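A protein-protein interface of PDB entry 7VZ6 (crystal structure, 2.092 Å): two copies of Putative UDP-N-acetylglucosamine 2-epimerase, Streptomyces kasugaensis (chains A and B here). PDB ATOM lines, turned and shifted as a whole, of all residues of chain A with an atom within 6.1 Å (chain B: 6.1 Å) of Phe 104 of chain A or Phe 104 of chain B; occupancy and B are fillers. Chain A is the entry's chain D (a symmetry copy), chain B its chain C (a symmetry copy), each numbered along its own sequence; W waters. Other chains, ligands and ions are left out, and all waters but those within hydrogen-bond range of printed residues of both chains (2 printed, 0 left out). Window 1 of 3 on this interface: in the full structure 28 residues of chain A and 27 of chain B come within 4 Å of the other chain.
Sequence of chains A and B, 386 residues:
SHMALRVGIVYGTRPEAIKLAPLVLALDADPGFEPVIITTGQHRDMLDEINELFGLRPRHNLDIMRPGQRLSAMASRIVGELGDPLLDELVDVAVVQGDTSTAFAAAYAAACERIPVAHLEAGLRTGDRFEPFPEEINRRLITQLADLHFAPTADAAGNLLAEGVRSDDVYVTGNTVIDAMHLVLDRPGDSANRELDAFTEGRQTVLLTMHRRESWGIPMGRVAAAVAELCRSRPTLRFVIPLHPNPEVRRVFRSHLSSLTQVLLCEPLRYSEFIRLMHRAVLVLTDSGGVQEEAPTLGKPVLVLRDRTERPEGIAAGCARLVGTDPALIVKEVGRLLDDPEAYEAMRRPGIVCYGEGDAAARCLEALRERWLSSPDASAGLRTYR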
ATOM      1  N   ALA A  75     -16.125 -26.759 -14.177  1.00  0.00           N
ATOM      2  CA  ALA A  75     -16.979 -27.105 -13.020  1.00  0.00           C
ATOM      3  C   ALA A  75     -17.392 -28.594 -13.124  1.00  0.00           C
ATOM      4  O   ALA A  75     -17.302 -29.318 -12.126  1.00  0.00           O
ATOM      5  CB  ALA A  75     -18.150 -26.181 -12.952  1.00  0.00           C
ATOM      6  N   VAL A  79     -16.560 -31.292 -10.152  1.00  0.00           N
ATOM      7  CA  VAL A  79     -17.709 -32.024  -9.531  1.00  0.00           C
ATOM      8  C   VAL A  79     -17.500 -33.527  -9.764  1.00  0.00           C
ATOM      9  O   VAL A  79     -17.741 -34.312  -8.824  1.00  0.00           O
ATOM     10  CB  VAL A  79     -19.059 -31.553 -10.092  1.00  0.00           C
ATOM     11  CG1 VAL A  79     -20.204 -32.424  -9.588  1.00  0.00           C
ATOM     12  CG2 VAL A  79     -19.307 -30.095  -9.734  1.00  0.00           C
ATOM     13  N   VAL A  96     -12.745 -24.637   1.821  1.00  0.00           N
ATOM     14  CA  VAL A  96     -12.549 -23.857   0.569  1.00  0.00           C
ATOM     15  C   VAL A  96     -12.450 -22.391   0.975  1.00  0.00           C
ATOM     16  O   VAL A  96     -12.953 -22.026   2.043  1.00  0.00           O
ATOM     17  CB  VAL A  96     -13.679 -24.112  -0.452  1.00  0.00           C
ATOM     18  CG1 VAL A  96     -13.706 -25.549  -0.909  1.00  0.00           C
ATOM     19  CG2 VAL A  96     -15.035 -23.728   0.074  1.00  0.00           C
ATOM     20  N   ASP A  99     -13.929 -17.010  -3.570  1.00  0.00           N
ATOM     21  CA  ASP A  99     -15.073 -16.844  -4.503  1.00  0.00           C
ATOM     22  C   ASP A  99     -14.849 -17.639  -5.783  1.00  0.00           C
ATOM     23  O   ASP A  99     -15.581 -17.388  -6.746  1.00  0.00           O
ATOM     24  CB  ASP A  99     -15.281 -15.367  -4.797  1.00  0.00           C
ATOM     25  CG  ASP A  99     -14.112 -14.702  -5.509  1.00  0.00           C
ATOM     26  OD1 ASP A  99     -13.121 -15.428  -5.895  1.00  0.00           O
ATOM     27  OD2 ASP A  99     -14.175 -13.457  -5.677  1.00  0.00           O
ATOM     28  N   THR A 100     -13.866 -18.525  -5.835  1.00  0.00           N
ATOM     29  CA  THR A 100     -13.470 -19.197  -7.103  1.00  0.00           C
ATOM     30  C   THR A 100     -14.502 -20.267  -7.466  1.00  0.00           C
ATOM     31  O   THR A 100     -15.223 -20.773  -6.592  1.00  0.00           O
ATOM     32  CB  THR A 100     -12.080 -19.833  -7.017  1.00  0.00           C
ATOM     33  OG1 THR A 100     -12.089 -20.761  -5.939  1.00  0.00           O
ATOM     34  CG2 THR A 100     -10.989 -18.800  -6.826  1.00  0.00           C
ATOM     35  N   SER A 101     -14.510 -20.635  -8.731  1.00  0.00           N
ATOM     36  CA  SER A 101     -15.306 -21.764  -9.264  1.00  0.00           C
ATOM     37  C   SER A 101     -14.767 -23.076  -8.681  1.00  0.00           C
ATOM     38  O   SER A 101     -15.564 -23.989  -8.436  1.00  0.00           O
ATOM     39  CB  SER A 101     -15.310 -21.671 -10.761  1.00  0.00           C
ATOM     40  OG  SER A 101     -16.058 -20.513 -11.127  1.00  0.00           O
ATOM     41  N   THR A 102     -13.473 -23.145  -8.361  1.00  0.00           N
ATOM     42  CA  THR A 102     -12.891 -24.273  -7.589  1.00  0.00           C
ATOM     43  C   THR A 102     -13.565 -24.369  -6.229  1.00  0.00           C
ATOM     44  O   THR A 102     -13.945 -25.482  -5.833  1.00  0.00           O
ATOM     45  CB  THR A 102     -11.375 -24.129  -7.387  1.00  0.00           C
ATOM     46  OG1 THR A 102     -10.781 -24.436  -8.641  1.00  0.00           O
ATOM     47  CG2 THR A 102     -10.812 -25.077  -6.358  1.00  0.00           C
ATOM     48  N   ALA A 103     -13.649 -23.259  -5.499  1.00  0.00           N
ATOM     49  CA  ALA A 103     -14.231 -23.257  -4.150  1.00  0.00           C
ATOM     50  C   ALA A 103     -15.666 -23.778  -4.252  1.00  0.00           C
ATOM     51  O   ALA A 103     -16.051 -24.592  -3.404  1.00  0.00           O
ATOM     52  CB  ALA A 103     -14.160 -21.898  -3.537  1.00  0.00           C
ATOM     53  N   PHE A 104     -16.435 -23.332  -5.253  1.00  0.00           N
ATOM     54  CA  PHE A 104     -17.857 -23.737  -5.371  1.00  0.00           C
ATOM     55  C   PHE A 104     -17.932 -25.209  -5.755  1.00  0.00           C
ATOM     56  O   PHE A 104     -18.602 -25.984  -5.062  1.00  0.00           O
ATOM     57  CB  PHE A 104     -18.623 -22.890  -6.391  1.00  0.00           C
ATOM     58  CG  PHE A 104     -19.839 -23.616  -6.907  1.00  0.00           C
ATOM     59  CD1 PHE A 104     -20.829 -24.024  -6.040  1.00  0.00           C
ATOM     60  CD2 PHE A 104     -19.915 -24.010  -8.223  1.00  0.00           C
ATOM     61  CE1 PHE A 104     -21.914 -24.746  -6.500  1.00  0.00           C
ATOM     62  CE2 PHE A 104     -20.983 -24.760  -8.676  1.00  0.00           C
ATOM     63  CZ  PHE A 104     -21.995 -25.100  -7.815  1.00  0.00           C
ATOM     64  N   ALA A 105     -17.283 -25.594  -6.860  1.00  0.00           N
ATOM     65  CA  ALA A 105     -17.358 -26.977  -7.391  1.00  0.00           C
ATOM     66  C   ALA A 105     -16.803 -27.974  -6.367  1.00  0.00           C
ATOM     67  O   ALA A 105     -17.403 -29.053  -6.221  1.00  0.00           O
ATOM     68  CB  ALA A 105     -16.651 -27.074  -8.714  1.00  0.00           C
ATOM     69  N   ALA A 106     -15.745 -27.621  -5.637  1.00  0.00           N
ATOM     70  CA  ALA A 106     -15.155 -28.488  -4.592  1.00  0.00           C
ATOM     71  C   ALA A 106     -16.115 -28.607  -3.397  1.00  0.00           C
ATOM     72  O   ALA A 106     -16.243 -29.723  -2.827  1.00  0.00           O
ATOM     73  CB  ALA A 106     -13.802 -27.965  -4.165  1.00  0.00           C
ATOM     74  N   ALA A 107     -16.759 -27.511  -2.989  1.00  0.00           N
ATOM     75  CA  ALA A 107     -17.748 -27.577  -1.893  1.00  0.00           C
ATOM     76  C   ALA A 107     -18.860 -28.539  -2.301  1.00  0.00           C
ATOM     77  O   ALA A 107     -19.292 -29.354  -1.456  1.00  0.00           O
ATOM     78  CB  ALA A 107     -18.260 -26.198  -1.541  1.00  0.00           C
ATOM     79  N   TYR A 108     -19.299 -28.475  -3.565  1.00  0.00           N
ATOM     80  CA  TYR A 108     -20.415 -29.326  -4.030  1.00  0.00           C
ATOM     81  C   TYR A 108     -19.947 -30.792  -4.050  1.00  0.00           C
ATOM     82  O   TYR A 108     -20.700 -31.697  -3.601  1.00  0.00           O
ATOM     83  CB  TYR A 108     -20.985 -28.870  -5.368  1.00  0.00           C
ATOM     84  CG  TYR A 108     -22.124 -29.743  -5.824  1.00  0.00           C
ATOM     85  CD1 TYR A 108     -23.379 -29.690  -5.229  1.00  0.00           C
ATOM     86  CD2 TYR A 108     -21.926 -30.685  -6.815  1.00  0.00           C
ATOM     87  CE1 TYR A 108     -24.417 -30.518  -5.636  1.00  0.00           C
ATOM     88  CE2 TYR A 108     -22.946 -31.530  -7.215  1.00  0.00           C
ATOM     89  CZ  TYR A 108     -24.193 -31.455  -6.626  1.00  0.00           C
ATOM     90  OH  TYR A 108     -25.154 -32.311  -7.106  1.00  0.00           O
ATOM     91  N   ALA A 109     -18.753 -31.030  -4.587  1.00  0.00           N
ATOM     92  CA  ALA A 109     -18.169 -32.388  -4.689  1.00  0.00           C
ATOM     93  C   ALA A 109     -18.065 -32.975  -3.274  1.00  0.00           C
ATOM     94  O   ALA A 109     -18.456 -34.172  -3.093  1.00  0.00           O
ATOM     95  CB  ALA A 109     -16.844 -32.346  -5.402  1.00  0.00           C
ATOM     96  N   ASN A 138     -20.855 -17.606  -6.986  1.00  0.00           N
ATOM     97  CA  ASN A 138     -20.054 -18.669  -6.316  1.00  0.00           C
ATOM     98  C   ASN A 138     -20.155 -18.492  -4.794  1.00  0.00           C
ATOM     99  O   ASN A 138     -20.394 -19.492  -4.115  1.00  0.00           O
ATOM    100  CB  ASN A 138     -18.599 -18.659  -6.774  1.00  0.00           C
ATOM    101  CG  ASN A 138     -18.410 -19.171  -8.179  1.00  0.00           C
ATOM    102  OD1 ASN A 138     -19.237 -19.914  -8.715  1.00  0.00           O
ATOM    103  ND2 ASN A 138     -17.277 -18.820  -8.760  1.00  0.00           N
ATOM    104  N   LEU A 141     -23.580 -19.600  -3.482  1.00  0.00           N
ATOM    105  CA  LEU A 141     -23.686 -21.076  -3.555  1.00  0.00           C
ATOM    106  C   LEU A 141     -22.855 -21.726  -2.439  1.00  0.00           C
ATOM    107  O   LEU A 141     -23.382 -22.579  -1.710  1.00  0.00           O
ATOM    108  CB  LEU A 141     -23.249 -21.546  -4.934  1.00  0.00           C
ATOM    109  CG  LEU A 141     -24.153 -21.136  -6.097  1.00  0.00           C
ATOM    110  CD1 LEU A 141     -23.511 -21.511  -7.408  1.00  0.00           C
ATOM    111  CD2 LEU A 141     -25.518 -21.769  -5.994  1.00  0.00           C
ATOM    112  N   ILE A 142     -21.617 -21.335  -2.284  1.00  0.00           N
ATOM    113  CA  ILE A 142     -20.744 -21.864  -1.185  1.00  0.00           C
ATOM    114  C   ILE A 142     -21.440 -21.608   0.159  1.00  0.00           C
ATOM    115  O   ILE A 142     -21.438 -22.498   1.012  1.00  0.00           O
ATOM    116  CB  ILE A 142     -19.341 -21.220  -1.229  1.00  0.00           C
ATOM    117  CG1 ILE A 142     -18.608 -21.562  -2.516  1.00  0.00           C
ATOM    118  CG2 ILE A 142     -18.541 -21.642  -0.005  1.00  0.00           C
ATOM    119  CD1 ILE A 142     -17.460 -20.640  -2.828  1.00  0.00           C
ATOM    120  N   LEU A 145     -23.830 -24.269   0.880  1.00  0.00           N
ATOM    121  CA  LEU A 145     -23.211 -25.607   1.026  1.00  0.00           C
ATOM    122  C   LEU A 145     -22.458 -25.725   2.350  1.00  0.00           C
ATOM    123  O   LEU A 145     -22.383 -26.849   2.852  1.00  0.00           O
ATOM    124  CB  LEU A 145     -22.260 -25.860  -0.139  1.00  0.00           C
ATOM    125  CG  LEU A 145     -22.957 -26.198  -1.442  1.00  0.00           C
ATOM    126  CD1 LEU A 145     -22.060 -25.938  -2.623  1.00  0.00           C
ATOM    127  CD2 LEU A 145     -23.403 -27.646  -1.414  1.00  0.00           C
ATOM    128  N   ALA B  75     -24.517 -35.147 -11.631  1.00  0.00           N
ATOM    129  CA  ALA B  75     -24.440 -33.663 -11.619  1.00  0.00           C
ATOM    130  C   ALA B  75     -23.339 -33.205 -12.594  1.00  0.00           C
ATOM    131  O   ALA B  75     -23.589 -32.288 -13.401  1.00  0.00           O
ATOM    132  CB  ALA B  75     -24.213 -33.162 -10.220  1.00  0.00           C
ATOM    133  N   VAL B  79     -24.099 -30.659 -15.729  1.00  0.00           N
ATOM    134  CA  VAL B  79     -23.312 -29.389 -15.796  1.00  0.00           C
ATOM    135  C   VAL B  79     -22.505 -29.379 -17.102  1.00  0.00           C
ATOM    136  O   VAL B  79     -22.463 -28.320 -17.763  1.00  0.00           O
ATOM    137  CB  VAL B  79     -22.402 -29.213 -14.570  1.00  0.00           C
ATOM    138  CG1 VAL B  79     -21.473 -28.011 -14.729  1.00  0.00           C
ATOM    139  CG2 VAL B  79     -23.224 -29.096 -13.295  1.00  0.00           C
ATOM    140  N   VAL B  96     -36.692 -24.325 -14.302  1.00  0.00           N
ATOM    141  CA  VAL B  96     -36.555 -25.615 -13.582  1.00  0.00           C
ATOM    142  C   VAL B  96     -37.620 -25.644 -12.488  1.00  0.00           C
ATOM    143  O   VAL B  96     -38.092 -24.583 -12.067  1.00  0.00           O
ATOM    144  CB  VAL B  96     -35.132 -25.799 -13.011  1.00  0.00           C
ATOM    145  CG1 VAL B  96     -34.110 -25.887 -14.114  1.00  0.00           C
ATOM    146  CG2 VAL B  96     -34.768 -24.718 -11.994  1.00  0.00           C
ATOM    147  N   ASP B  99     -37.093 -29.761  -6.607  1.00  0.00           N
ATOM    148  CA  ASP B  99     -35.949 -29.944  -5.701  1.00  0.00           C
ATOM    149  C   ASP B  99     -34.942 -30.936  -6.278  1.00  0.00           C
ATOM    150  O   ASP B  99     -34.080 -31.377  -5.522  1.00  0.00           O
ATOM    151  CB  ASP B  99     -36.448 -30.399  -4.324  1.00  0.00           C
ATOM    152  CG  ASP B  99     -37.145 -31.747  -4.333  1.00  0.00           C
ATOM    153  OD1 ASP B  99     -37.176 -32.415  -5.414  1.00  0.00           O
ATOM    154  OD2 ASP B  99     -37.664 -32.133  -3.264  1.00  0.00           O
ATOM    155  N   THR B 100     -35.065 -31.328  -7.530  1.00  0.00           N
ATOM    156  CA  THR B 100     -34.248 -32.433  -8.110  1.00  0.00           C
ATOM    157  C   THR B 100     -32.812 -31.948  -8.353  1.00  0.00           C
ATOM    158  O   THR B 100     -32.570 -30.726  -8.490  1.00  0.00           O
ATOM    159  CB  THR B 100     -34.828 -32.964  -9.420  1.00  0.00           C
ATOM    160  OG1 THR B 100     -34.932 -31.863 -10.326  1.00  0.00           O
ATOM    161  CG2 THR B 100     -36.183 -33.619  -9.218  1.00  0.00           C
ATOM    162  N   SER B 101     -31.900 -32.891  -8.455  1.00  0.00           N
ATOM    163  CA  SER B 101     -30.499 -32.657  -8.857  1.00  0.00           C
ATOM    164  C   SER B 101     -30.463 -32.180 -10.316  1.00  0.00           C
ATOM    165  O   SER B 101     -29.611 -31.337 -10.648  1.00  0.00           O
ATOM    166  CB  SER B 101     -29.680 -33.869  -8.547  1.00  0.00           C
ATOM    167  OG  SER B 101     -29.630 -34.034  -7.128  1.00  0.00           O
ATOM    168  N   THR B 102     -31.427 -32.590 -11.133  1.00  0.00           N
ATOM    169  CA  THR B 102     -31.634 -32.022 -12.492  1.00  0.00           C
ATOM    170  C   THR B 102     -31.901 -30.528 -12.403  1.00  0.00           C
ATOM    171  O   THR B 102     -31.269 -29.761 -13.157  1.00  0.00           O
ATOM    172  CB  THR B 102     -32.780 -32.701 -13.250  1.00  0.00           C
ATOM    173  OG1 THR B 102     -32.304 -33.985 -13.631  1.00  0.00           O
ATOM    174  CG2 THR B 102     -33.158 -31.960 -14.504  1.00  0.00           C
ATOM    175  N   ALA B 103     -32.852 -30.127 -11.553  1.00  0.00           N
ATOM    176  CA  ALA B 103     -33.224 -28.712 -11.421  1.00  0.00           C
ATOM    177  C   ALA B 103     -31.976 -27.921 -11.035  1.00  0.00           C
ATOM    178  O   ALA B 103     -31.761 -26.850 -11.613  1.00  0.00           O
ATOM    179  CB  ALA B 103     -34.341 -28.526 -10.434  1.00  0.00           C
ATOM    180  N   PHE B 104     -31.174 -28.426 -10.089  1.00  0.00           N
ATOM    181  CA  PHE B 104     -29.989 -27.680  -9.596  1.00  0.00           C
ATOM    182  C   PHE B 104     -28.936 -27.626 -10.699  1.00  0.00           C
ATOM    183  O   PHE B 104     -28.483 -26.533 -11.055  1.00  0.00           O
ATOM    184  CB  PHE B 104     -29.396 -28.281  -8.327  1.00  0.00           C
ATOM    185  CG  PHE B 104     -27.948 -27.903  -8.159  1.00  0.00           C
ATOM    186  CD1 PHE B 104     -27.583 -26.578  -8.058  1.00  0.00           C
ATOM    187  CD2 PHE B 104     -26.958 -28.859  -8.244  1.00  0.00           C
ATOM    188  CE1 PHE B 104     -26.247 -26.218  -7.977  1.00  0.00           C
ATOM    189  CE2 PHE B 104     -25.620 -28.497  -8.177  1.00  0.00           C
ATOM    190  CZ  PHE B 104     -25.268 -27.182  -8.040  1.00  0.00           C
ATOM    191  N   ALA B 105     -28.529 -28.777 -11.220  1.00  0.00           N
ATOM    192  CA  ALA B 105     -27.438 -28.881 -12.217  1.00  0.00           C
ATOM    193  C   ALA B 105     -27.822 -28.135 -13.494  1.00  0.00           C
ATOM    194  O   ALA B 105     -26.937 -27.463 -14.070  1.00  0.00           O
ATOM    195  CB  ALA B 105     -27.106 -30.316 -12.479  1.00  0.00           C
ATOM    196  N   ALA B 106     -29.088 -28.177 -13.910  1.00  0.00           N
ATOM    197  CA  ALA B 106     -29.568 -27.446 -15.103  1.00  0.00           C
ATOM    198  C   ALA B 106     -29.558 -25.940 -14.845  1.00  0.00           C
ATOM    199  O   ALA B 106     -29.187 -25.159 -15.764  1.00  0.00           O
ATOM    200  CB  ALA B 106     -30.930 -27.936 -15.508  1.00  0.00           C
ATOM    201  N   ALA B 107     -29.966 -25.493 -13.651  1.00  0.00           N
ATOM    202  CA  ALA B 107     -29.928 -24.064 -13.321  1.00  0.00           C
ATOM    203  C   ALA B 107     -28.475 -23.596 -13.413  1.00  0.00           C
ATOM    204  O   ALA B 107     -28.237 -22.492 -13.958  1.00  0.00           O
ATOM    205  CB  ALA B 107     -30.554 -23.794 -11.984  1.00  0.00           C
ATOM    206  N   TYR B 108     -27.530 -24.405 -12.921  1.00  0.00           N
ATOM    207  CA  TYR B 108     -26.103 -24.012 -12.923  1.00  0.00           C
ATOM    208  C   TYR B 108     -25.600 -23.958 -14.373  1.00  0.00           C
ATOM    209  O   TYR B 108     -24.894 -22.993 -14.752  1.00  0.00           O
ATOM    210  CB  TYR B 108     -25.253 -24.916 -12.031  1.00  0.00           C
ATOM    211  CG  TYR B 108     -23.805 -24.504 -12.029  1.00  0.00           C
ATOM    212  CD1 TYR B 108     -23.383 -23.374 -11.358  1.00  0.00           C
ATOM    213  CD2 TYR B 108     -22.868 -25.196 -12.775  1.00  0.00           C
ATOM    214  CE1 TYR B 108     -22.050 -22.978 -11.352  1.00  0.00           C
ATOM    215  CE2 TYR B 108     -21.547 -24.799 -12.822  1.00  0.00           C
ATOM    216  CZ  TYR B 108     -21.132 -23.695 -12.102  1.00  0.00           C
ATOM    217  OH  TYR B 108     -19.819 -23.321 -12.147  1.00  0.00           O
ATOM    218  N   ALA B 109     -25.927 -24.978 -15.167  1.00  0.00           N
ATOM    219  CA  ALA B 109     -25.503 -25.067 -16.578  1.00  0.00           C
ATOM    220  C   ALA B 109     -26.048 -23.844 -17.335  1.00  0.00           C
ATOM    221  O   ALA B 109     -25.271 -23.229 -18.109  1.00  0.00           O
ATOM    222  CB  ALA B 109     -25.950 -26.373 -17.176  1.00  0.00           C
ATOM    223  N   ASN B 138     -30.463 -28.735  -2.703  1.00  0.00           N
ATOM    224  CA  ASN B 138     -30.784 -28.389  -4.104  1.00  0.00           C
ATOM    225  C   ASN B 138     -31.649 -27.121  -4.130  1.00  0.00           C
ATOM    226  O   ASN B 138     -31.317 -26.213  -4.905  1.00  0.00           O
ATOM    227  CB  ASN B 138     -31.461 -29.528  -4.849  1.00  0.00           C
ATOM    228  CG  ASN B 138     -30.522 -30.676  -5.160  1.00  0.00           C
ATOM    229  OD1 ASN B 138     -29.287 -30.518  -5.191  1.00  0.00           O
ATOM    230  ND2 ASN B 138     -31.113 -31.821  -5.434  1.00  0.00           N
ATOM    231  N   LEU B 141     -29.605 -23.971  -3.280  1.00  0.00           N
ATOM    232  CA  LEU B 141     -28.697 -23.643  -4.409  1.00  0.00           C
ATOM    233  C   LEU B 141     -29.498 -23.038  -5.582  1.00  0.00           C
ATOM    234  O   LEU B 141     -29.120 -21.972  -6.076  1.00  0.00           O
ATOM    235  CB  LEU B 141     -27.958 -24.905  -4.844  1.00  0.00           C
ATOM    236  CG  LEU B 141     -26.965 -25.474  -3.838  1.00  0.00           C
ATOM    237  CD1 LEU B 141     -26.461 -26.819  -4.318  1.00  0.00           C
ATOM    238  CD2 LEU B 141     -25.801 -24.524  -3.646  1.00  0.00           C
ATOM    239  N   ILE B 142     -30.590 -23.662  -5.977  1.00  0.00           N
ATOM    240  CA  ILE B 142     -31.460 -23.119  -7.054  1.00  0.00           C
ATOM    241  C   ILE B 142     -31.904 -21.705  -6.658  1.00  0.00           C
ATOM    242  O   ILE B 142     -31.918 -20.817  -7.518  1.00  0.00           O
ATOM    243  CB  ILE B 142     -32.670 -24.034  -7.320  1.00  0.00           C
ATOM    244  CG1 ILE B 142     -32.245 -25.399  -7.835  1.00  0.00           C
ATOM    245  CG2 ILE B 142     -33.635 -23.366  -8.287  1.00  0.00           C
ATOM    246  CD1 ILE B 142     -33.299 -26.476  -7.666  1.00  0.00           C
ATOM    247  N   LEU B 145     -29.378 -19.263  -7.606  1.00  0.00           N
ATOM    248  CA  LEU B 145     -29.130 -19.201  -9.065  1.00  0.00           C
ATOM    249  C   LEU B 145     -30.280 -18.510  -9.800  1.00  0.00           C
ATOM    250  O   LEU B 145     -29.985 -17.865 -10.836  1.00  0.00           O
ATOM    251  CB  LEU B 145     -28.959 -20.599  -9.626  1.00  0.00           C
ATOM    252  CG  LEU B 145     -27.597 -21.223  -9.324  1.00  0.00           C
ATOM    253  CD1 LEU B 145     -27.673 -22.724  -9.450  1.00  0.00           C
ATOM    254  CD2 LEU B 145     -26.531 -20.634 -10.234  1.00  0.00           C
HETATM  255  O   HOH W   1     -27.671 -32.225  -6.238  1.00  0.00           O
HETATM  256  O   HOH W   2     -18.790 -21.213 -11.070  1.00  0.00           O
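Thr 100 of chain A touches none of the printed residues of chain B. Of chain B, only Phe 104 and Tyr 108 come within 4 Å of Phe 104 of chain A. Printed residues of chain B within 4 Å of Tyr 108 of chain A: Ala 75 and Phe 104. Printed residues of chain B within 4 Å of Leu 145 of chain A: Leu 141 (3.97 Å). Of chain A, only Phe 104 and Tyr 108 come within 4 Å of Phe 104 of chain B. Of the printed residues of chain A, Tyr 108 of chain B touches Ala 75 (3.4 Å) and Phe 104 (3.4 Å). Printed residues of chain A within 4 Å of Leu 141 of chain B: Leu 141 (3.6 Å) and Leu 145 (3.97 Å). The nearest residue of chain A that does not touch Phe 104 of chain B is Leu 141 of chain A (4.9 Å).
Ala 75 of chain A touches Tyr 108 of chain B, and with the chains exchanged Tyr 108 of chain A touches Ala 75 of chain B. Phe 104 of chain A touches Tyr 108 of chain B, and with the chains exchanged Tyr 108 of chain A touches Phe 104 of chain B. Leu 141 of chain B touches its own counterpart, Leu 141 of chain A. Leu 141 of chain A touches Leu 145 of chain B, and with the chains exchanged Leu 145 of chain A touches Leu 141 of chain B. Positions printed for both chains: 75, 79, 96, 99, 100, 101, 102, 103, 104, 105, 106, 107, 108, 109, 138, 141, 142 and 145. Of the 8 pairs that touch across the chains among the printed residues, 8 have their exchanged pair printed and touching as well.
Water W1 lies within hydrogen-bond range of OD1 of Asn 138 of chain B (2.6 Å), OH of Tyr 108 of chain A (2.7 Å) and OG of Ser 101 of chain B (2.8 Å). Water W2 lies within hydrogen-bond range of the side-chain hydroxyl (OH) of Tyr 108 of chain B (2.6 Å), the side-chain amide oxygen (OD1) of Asn 138 of chain A (2.7 Å) and the side-chain hydroxyl (OG) of Ser 101 of chain A (2.8 Å).
Of the 18 printed residues of chain A, 5 touch a printed residue of chain B. Among the printed residues, 8 pairs touch across the chains. Among the printed residues, no Asp or Glu carboxylate lies within 4 Å of a Lys or Arg side-chain nitrogen of the other chain.
Among the printed residues, merely in contact across the chains: Tyr 108 of chain A with Ala 75 of chain B (3.4 Å), Phe 104 of chain A with Tyr 108 of chain B (3.4 Å), Ala 75 of chain A with Tyr 108 of chain B (3.4 Å), Tyr 108 of chain A with Phe 104 of chain B (3.5 Å), Leu 141 of chain A with Leu 141 of chain B (3.6 Å), Phe 104 of chain A with Phe 104 of chain B (3.9 Å), Leu 141 of chain A with Leu 145 of chain B (3.96 Å) and Leu 145 of chain A with Leu 141 of chain B (3.97 Å).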
